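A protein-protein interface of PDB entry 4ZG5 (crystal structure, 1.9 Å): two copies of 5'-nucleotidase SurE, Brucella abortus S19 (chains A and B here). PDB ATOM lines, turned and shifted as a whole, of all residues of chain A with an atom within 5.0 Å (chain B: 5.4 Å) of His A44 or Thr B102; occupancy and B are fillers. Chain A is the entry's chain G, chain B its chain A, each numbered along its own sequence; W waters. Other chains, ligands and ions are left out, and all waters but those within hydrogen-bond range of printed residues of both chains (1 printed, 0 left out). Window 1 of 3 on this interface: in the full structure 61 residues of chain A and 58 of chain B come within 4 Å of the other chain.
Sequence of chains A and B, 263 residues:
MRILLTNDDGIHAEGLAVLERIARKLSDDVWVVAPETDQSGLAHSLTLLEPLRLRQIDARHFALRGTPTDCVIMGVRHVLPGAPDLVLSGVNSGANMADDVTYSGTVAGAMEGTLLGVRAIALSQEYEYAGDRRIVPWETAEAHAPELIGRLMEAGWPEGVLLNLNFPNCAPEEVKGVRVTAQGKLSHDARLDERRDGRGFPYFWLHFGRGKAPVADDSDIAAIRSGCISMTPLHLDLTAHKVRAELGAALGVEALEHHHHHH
Thr B102 touches one residue of chain A. Printed residues of chain B within 4 Å of Leu A46: Gly B41 and Tyr B103. Printed residues of chain A within 4 Å of Leu B42: Ser A45. Ala B98 touches none of the printed residues of chain A. Ala A108 touches none of the printed residues of chain B. The nearest residue of chain B that does not touch His A44 is Gly B41 (4.6 Å). The nearest residue of chain A that does not touch Thr B102 is Met A111 (4.5 Å).
Ala A43 touches His B44, and with the chains exchanged His A44 touches Ala B43. Positions printed for both chains: 42, 43, 44, 104 and 111. Of the 12 pairs that touch across the chains among the printed residues, 2 have their exchanged pair printed and touching as well.
The side-chain carboxylate of Glu A112 sits at hydrogen-bond distance from the side-chain hydroxyl of Tyr B103. The backbone NH (N) of Leu A46 is in hydrogen-bond range of the backbone carbonyl oxygen (O) of Gly B41.
Ala A43 touches His B44. Ala B43 touches His A44 (CB to C, 3.5 Å). CG2 of Thr B102 touches ND1 of His A44, at 2.8 Å. Tyr B103 touches His A44 (CE1 to CE1, 3.1 Å). Gly B41 touches Ser A45. Leu B42 touches Ser A45. Ser A45 touches Ala B43 (N to CB, 3.6 Å). Leu A46 touches Tyr B103. Asp B99 touches Leu A115 (OD2 to CD2, 3.5 Å). Leu A115 touches Tyr B103 (CD1 to OH, 3.3 Å).
The side-chain hydroxyl of Thr B102 is in hydrogen-bond range of the backbone carbonyl oxygen of Asp B99, at 2.9 Å. The side-chain carboxylate of Glu A112 lies within hydrogen-bond range of a ring nitrogen (NE2) of His A44 (2.6 Å). N of Ala B43 lies within hydrogen-bond range of O of Tyr B103. The backbone carbonyl oxygen (O) of Leu A42 sits at hydrogen-bond distance from the side-chain hydroxyl (OG) of Ser A45 (2.6 Å).
Water W1 lies within hydrogen-bond range of the backbone NH (N) of His A44 (2.9 Å), the backbone NH (N) of His B44 (3.2 Å) and the backbone carbonyl oxygen (O) of Thr B102 (3.3 Å).
Of the 11 printed residues of chain A, 6 touch a printed residue of chain B. Hydrophobic or aromatic side chains of chain A that line the printed part of chain B: Ala A43, His A44, Leu A46 and Leu A115. Hydrophobic or aromatic side chains of chain B within 4 Å of the printed part of chain A: Ala B43 and Tyr B103. Among the printed residues, 12 pairs touch across the chains. Among the printed residues, no Asp or Glu carboxylate lies within 4 Å of a Lys or Arg side-chain nitrogen of the other chain.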
ATOM      1  N   LEU A  42      -5.093  -2.803  24.225  1.00  0.00           N
ATOM      2  CA  LEU A  42      -4.531  -1.820  25.150  1.00  0.00           C
ATOM      3  C   LEU A  42      -3.606  -0.798  24.460  1.00  0.00           C
ATOM      4  O   LEU A  42      -3.231   0.208  25.101  1.00  0.00           O
ATOM      5  CB  LEU A  42      -3.871  -2.519  26.335  1.00  0.00           C
ATOM      6  CG  LEU A  42      -4.719  -2.684  27.633  1.00  0.00           C
ATOM      7  CD1 LEU A  42      -6.134  -3.205  27.537  1.00  0.00           C
ATOM      8  CD2 LEU A  42      -3.916  -3.630  28.480  1.00  0.00           C
ATOM      9  N   ALA A  43      -3.247  -1.085  23.207  1.00  0.00           N
ATOM     10  CA  ALA A  43      -2.523  -0.185  22.368  1.00  0.00           C
ATOM     11  C   ALA A  43      -1.205   0.252  23.031  1.00  0.00           C
ATOM     12  O   ALA A  43      -0.473  -0.600  23.539  1.00  0.00           O
ATOM     13  CB  ALA A  43      -3.435   0.985  22.001  1.00  0.00           C
ATOM     14  N   HIS A  44      -0.934   1.562  23.075  1.00  0.00           N
ATOM     15  CA  HIS A  44       0.280   2.091  23.643  1.00  0.00           C
ATOM     16  C   HIS A  44      -0.057   2.746  24.967  1.00  0.00           C
ATOM     17  O   HIS A  44       0.617   3.687  25.381  1.00  0.00           O
ATOM     18  CB  HIS A  44       1.038   3.025  22.669  1.00  0.00           C
ATOM     19  CG  HIS A  44       2.473   3.301  23.025  1.00  0.00           C
ATOM     20  ND1 HIS A  44       3.138   4.419  22.586  1.00  0.00           N
ATOM     21  CD2 HIS A  44       3.376   2.615  23.789  1.00  0.00           C
ATOM     22  CE1 HIS A  44       4.389   4.407  23.039  1.00  0.00           C
ATOM     23  NE2 HIS A  44       4.561   3.309  23.760  1.00  0.00           N
ATOM     24  N   SER A  45      -1.060   2.225  25.681  1.00  0.00           N
ATOM     25  CA  SER A  45      -1.485   2.843  26.952  1.00  0.00           C
ATOM     26  C   SER A  45      -0.481   2.414  28.028  1.00  0.00           C
ATOM     27  O   SER A  45       0.191   1.364  27.962  1.00  0.00           O
ATOM     28  CB  SER A  45      -2.908   2.367  27.393  1.00  0.00           C
ATOM     29  OG  SER A  45      -2.860   0.930  27.582  1.00  0.00           O
ATOM     30  N   LEU A  46      -0.392   3.266  29.000  1.00  0.00           N
ATOM     31  CA  LEU A  46       0.383   2.909  30.194  1.00  0.00           C
ATOM     32  C   LEU A  46      -0.342   3.311  31.460  1.00  0.00           C
ATOM     33  O   LEU A  46      -1.444   3.831  31.381  1.00  0.00           O
ATOM     34  CB  LEU A  46       1.795   3.474  30.073  1.00  0.00           C
ATOM     35  CG  LEU A  46       1.917   4.815  29.428  1.00  0.00           C
ATOM     36  CD1 LEU A  46       1.208   5.843  30.281  1.00  0.00           C
ATOM     37  CD2 LEU A  46       3.412   5.103  29.317  1.00  0.00           C
ATOM     38  N   THR A  69       3.530  -1.801  27.530  1.00  0.00           N
ATOM     39  CA  THR A  69       4.326  -0.598  27.558  1.00  0.00           C
ATOM     40  C   THR A  69       4.909  -0.384  28.934  1.00  0.00           C
ATOM     41  O   THR A  69       6.134  -0.164  29.104  1.00  0.00           O
ATOM     42  CB  THR A  69       3.439   0.563  27.149  1.00  0.00           C
ATOM     43  OG1 THR A  69       2.973   0.318  25.825  1.00  0.00           O
ATOM     44  CG2 THR A  69       4.205   1.846  27.181  1.00  0.00           C
ATOM     45  N   SER A 104      -2.737  -2.449  18.941  1.00  0.00           N
ATOM     46  CA  SER A 104      -2.013  -3.620  19.434  1.00  0.00           C
ATOM     47  C   SER A 104      -1.060  -3.352  20.615  1.00  0.00           C
ATOM     48  O   SER A 104      -0.104  -2.559  20.488  1.00  0.00           O
ATOM     49  CB  SER A 104      -1.184  -4.185  18.300  1.00  0.00           C
ATOM     50  OG  SER A 104      -0.341  -5.240  18.749  1.00  0.00           O
ATOM     51  N   ALA A 108       2.855  -2.221  20.616  1.00  0.00           N
ATOM     52  CA  ALA A 108       3.213  -1.087  21.487  1.00  0.00           C
ATOM     53  C   ALA A 108       4.426  -1.430  22.331  1.00  0.00           C
ATOM     54  O   ALA A 108       5.221  -0.586  22.662  1.00  0.00           O
ATOM     55  CB  ALA A 108       2.060  -0.784  22.368  1.00  0.00           C
ATOM     56  N   MET A 111       7.132  -0.567  20.161  1.00  0.00           N
ATOM     57  CA  MET A 111       7.218   0.895  20.048  1.00  0.00           C
ATOM     58  C   MET A 111       7.914   1.496  21.234  1.00  0.00           C
ATOM     59  O   MET A 111       8.807   2.367  21.125  1.00  0.00           O
ATOM     60  CB  MET A 111       5.848   1.550  20.013  1.00  0.00           C
ATOM     61  CG  MET A 111       4.936   1.069  18.921  1.00  0.00           C
ATOM     62  SD  MET A 111       3.363   1.977  19.066  1.00  0.00           S
ATOM     63  CE  MET A 111       2.608   1.626  17.498  1.00  0.00           C
ATOM     64  N   GLU A 112       7.552   1.004  22.403  1.00  0.00           N
ATOM     65  CA  GLU A 112       8.173   1.522  23.634  1.00  0.00           C
ATOM     66  C   GLU A 112       9.668   1.216  23.723  1.00  0.00           C
ATOM     67  O   GLU A 112      10.501   2.059  24.127  1.00  0.00           O
ATOM     68  CB  GLU A 112       7.449   0.947  24.887  1.00  0.00           C
ATOM     69  CG  GLU A 112       7.828   1.679  26.199  1.00  0.00           C
ATOM     70  CD  GLU A 112       7.478   3.131  26.165  1.00  0.00           C
ATOM     71  OE1 GLU A 112       6.632   3.556  25.361  1.00  0.00           O
ATOM     72  OE2 GLU A 112       8.171   3.903  26.901  1.00  0.00           O
ATOM     73  N   LEU A 115      11.255   3.756  21.621  1.00  0.00           N
ATOM     74  CA  LEU A 115      11.277   5.104  22.223  1.00  0.00           C
ATOM     75  C   LEU A 115      12.314   5.193  23.353  1.00  0.00           C
ATOM     76  O   LEU A 115      12.807   6.255  23.670  1.00  0.00           O
ATOM     77  CB  LEU A 115       9.925   5.502  22.768  1.00  0.00           C
ATOM     78  CG  LEU A 115       8.935   5.827  21.666  1.00  0.00           C
ATOM     79  CD1 LEU A 115       7.518   5.889  22.188  1.00  0.00           C
ATOM     80  CD2 LEU A 115       9.235   7.164  21.018  1.00  0.00           C
ATOM     81  N   GLY B  41      -2.934   8.832  29.798  1.00  0.00           N
ATOM     82  CA  GLY B  41      -2.081   7.698  29.381  1.00  0.00           C
ATOM     83  C   GLY B  41      -2.761   6.537  28.637  1.00  0.00           C
ATOM     84  O   GLY B  41      -2.204   5.478  28.518  1.00  0.00           O
ATOM     85  N   LEU B  42      -4.009   6.706  28.240  1.00  0.00           N
ATOM     86  CA  LEU B  42      -4.815   5.545  27.808  1.00  0.00           C
ATOM     87  C   LEU B  42      -4.658   5.366  26.336  1.00  0.00           C
ATOM     88  O   LEU B  42      -5.102   4.325  25.785  1.00  0.00           O
ATOM     89  CB  LEU B  42      -6.283   5.705  28.155  1.00  0.00           C
ATOM     90  CG  LEU B  42      -6.788   5.008  29.408  1.00  0.00           C
ATOM     91  CD1 LEU B  42      -5.999   5.181  30.678  1.00  0.00           C
ATOM     92  CD2 LEU B  42      -8.153   5.579  29.606  1.00  0.00           C
ATOM     93  N   ALA B  43      -3.979   6.336  25.685  1.00  0.00           N
ATOM     94  CA  ALA B  43      -3.582   6.239  24.311  1.00  0.00           C
ATOM     95  C   ALA B  43      -4.761   5.894  23.340  1.00  0.00           C
ATOM     96  O   ALA B  43      -5.785   6.594  23.353  1.00  0.00           O
ATOM     97  CB  ALA B  43      -2.447   5.224  24.207  1.00  0.00           C
ATOM     98  N   HIS B  44      -4.578   4.876  22.516  1.00  0.00           N
ATOM     99  CA  HIS B  44      -5.588   4.414  21.528  1.00  0.00           C
ATOM    100  C   HIS B  44      -6.175   3.112  22.063  1.00  0.00           C
ATOM    101  O   HIS B  44      -6.601   2.273  21.279  1.00  0.00           O
ATOM    102  CB  HIS B  44      -5.044   4.378  20.086  1.00  0.00           C
ATOM    103  CG  HIS B  44      -6.087   4.317  18.991  1.00  0.00           C
ATOM    104  ND1 HIS B  44      -5.878   3.652  17.806  1.00  0.00           N
ATOM    105  CD2 HIS B  44      -7.373   4.679  18.959  1.00  0.00           C
ATOM    106  CE1 HIS B  44      -6.945   3.756  17.038  1.00  0.00           C
ATOM    107  NE2 HIS B  44      -7.881   4.343  17.740  1.00  0.00           N
ATOM    108  N   ALA B  98       4.596  16.187  20.091  1.00  0.00           N
ATOM    109  CA  ALA B  98       5.813  15.411  20.029  1.00  0.00           C
ATOM    110  C   ALA B  98       5.548  13.929  20.375  1.00  0.00           C
ATOM    111  O   ALA B  98       4.547  13.390  19.944  1.00  0.00           O
ATOM    112  CB  ALA B  98       6.917  16.090  20.904  1.00  0.00           C
ATOM    113  N   ASP B  99       6.352  13.284  21.194  1.00  0.00           N
ATOM    114  CA  ASP B  99       6.081  11.870  21.559  1.00  0.00           C
ATOM    115  C   ASP B  99       4.777  11.634  22.429  1.00  0.00           C
ATOM    116  O   ASP B  99       4.350  10.517  22.550  1.00  0.00           O
ATOM    117  CB  ASP B  99       7.272  11.298  22.314  1.00  0.00           C
ATOM    118  CG  ASP B  99       8.493  11.245  21.457  1.00  0.00           C
ATOM    119  OD1 ASP B  99       9.382  12.043  21.730  1.00  0.00           O
ATOM    120  OD2 ASP B  99       8.513  10.522  20.427  1.00  0.00           O
ATOM    121  N   ASP B 100       4.139  12.685  22.957  1.00  0.00           N
ATOM    122  CA  ASP B 100       2.814  12.545  23.569  1.00  0.00           C
ATOM    123  C   ASP B 100       1.836  11.869  22.620  1.00  0.00           C
ATOM    124  O   ASP B 100       0.901  11.204  23.094  1.00  0.00           O
ATOM    125  CB  ASP B 100       2.136  13.848  23.990  1.00  0.00           C
ATOM    126  CG  ASP B 100       2.913  14.669  25.005  1.00  0.00           C
ATOM    127  OD1 ASP B 100       3.744  14.106  25.726  1.00  0.00           O
ATOM    128  OD2 ASP B 100       2.687  15.936  25.029  1.00  0.00           O
ATOM    129  N   VAL B 101       1.973  12.076  21.314  1.00  0.00           N
ATOM    130  CA  VAL B 101       0.856  11.751  20.427  1.00  0.00           C
ATOM    131  C   VAL B 101       0.431  10.252  20.445  1.00  0.00           C
ATOM    132  O   VAL B 101      -0.728   9.981  20.353  1.00  0.00           O
ATOM    133  CB  VAL B 101       1.024  12.234  18.927  1.00  0.00           C
ATOM    134  CG1 VAL B 101       1.362  13.710  18.826  1.00  0.00           C
ATOM    135  CG2 VAL B 101       2.004  11.411  18.157  1.00  0.00           C
ATOM    136  N   THR B 102       1.412   9.372  20.585  1.00  0.00           N
ATOM    137  CA  THR B 102       1.276   7.971  20.781  1.00  0.00           C
ATOM    138  C   THR B 102       0.503   7.556  22.026  1.00  0.00           C
ATOM    139  O   THR B 102      -0.042   6.453  22.113  1.00  0.00           O
ATOM    140  CB  THR B 102       2.751   7.395  21.119  1.00  0.00           C
ATOM    141  OG1 THR B 102       3.879   8.330  20.749  1.00  0.00           O
ATOM    142  CG2 THR B 102       2.813   6.247  20.538  1.00  0.00           C
ATOM    143  N   TYR B 103       0.663   8.346  23.051  1.00  0.00           N
ATOM    144  CA  TYR B 103       0.066   8.052  24.372  1.00  0.00           C
ATOM    145  C   TYR B 103      -1.226   8.760  24.704  1.00  0.00           C
ATOM    146  O   TYR B 103      -1.866   8.425  25.711  1.00  0.00           O
ATOM    147  CB  TYR B 103       1.066   8.407  25.473  1.00  0.00           C
ATOM    148  CG  TYR B 103       2.398   7.762  25.369  1.00  0.00           C
ATOM    149  CD1 TYR B 103       2.598   6.480  25.774  1.00  0.00           C
ATOM    150  CD2 TYR B 103       3.491   8.480  24.856  1.00  0.00           C
ATOM    151  CE1 TYR B 103       3.858   5.911  25.729  1.00  0.00           C
ATOM    152  CE2 TYR B 103       4.760   7.916  24.796  1.00  0.00           C
ATOM    153  CZ  TYR B 103       4.935   6.627  25.250  1.00  0.00           C
ATOM    154  OH  TYR B 103       6.182   6.098  25.202  1.00  0.00           O
ATOM    155  N   SER B 104      -1.604   9.725  23.873  1.00  0.00           N
ATOM    156  CA  SER B 104      -2.671  10.673  24.137  1.00  0.00           C
ATOM    157  C   SER B 104      -4.030  10.111  23.810  1.00  0.00           C
ATOM    158  O   SER B 104      -4.307   9.735  22.673  1.00  0.00           O
ATOM    159  CB  SER B 104      -2.479  11.939  23.291  1.00  0.00           C
ATOM    160  OG  SER B 104      -3.600  12.800  23.348  1.00  0.00           O
ATOM    161  N   MET B 111      -8.019  10.115  16.086  1.00  0.00           N
ATOM    162  CA  MET B 111      -7.650   8.975  15.290  1.00  0.00           C
ATOM    163  C   MET B 111      -8.775   8.067  14.942  1.00  0.00           C
ATOM    164  O   MET B 111      -8.880   7.552  13.798  1.00  0.00           O
ATOM    165  CB  MET B 111      -6.574   8.127  15.983  1.00  0.00           C
ATOM    166  CG  MET B 111      -5.314   8.835  16.382  1.00  0.00           C
ATOM    167  SD  MET B 111      -4.216   7.652  17.267  1.00  0.00           S
ATOM    168  CE  MET B 111      -2.658   8.497  17.261  1.00  0.00           C
HETATM  169  O   HOH W   1      -1.785   3.780  21.401  1.00  0.00           O
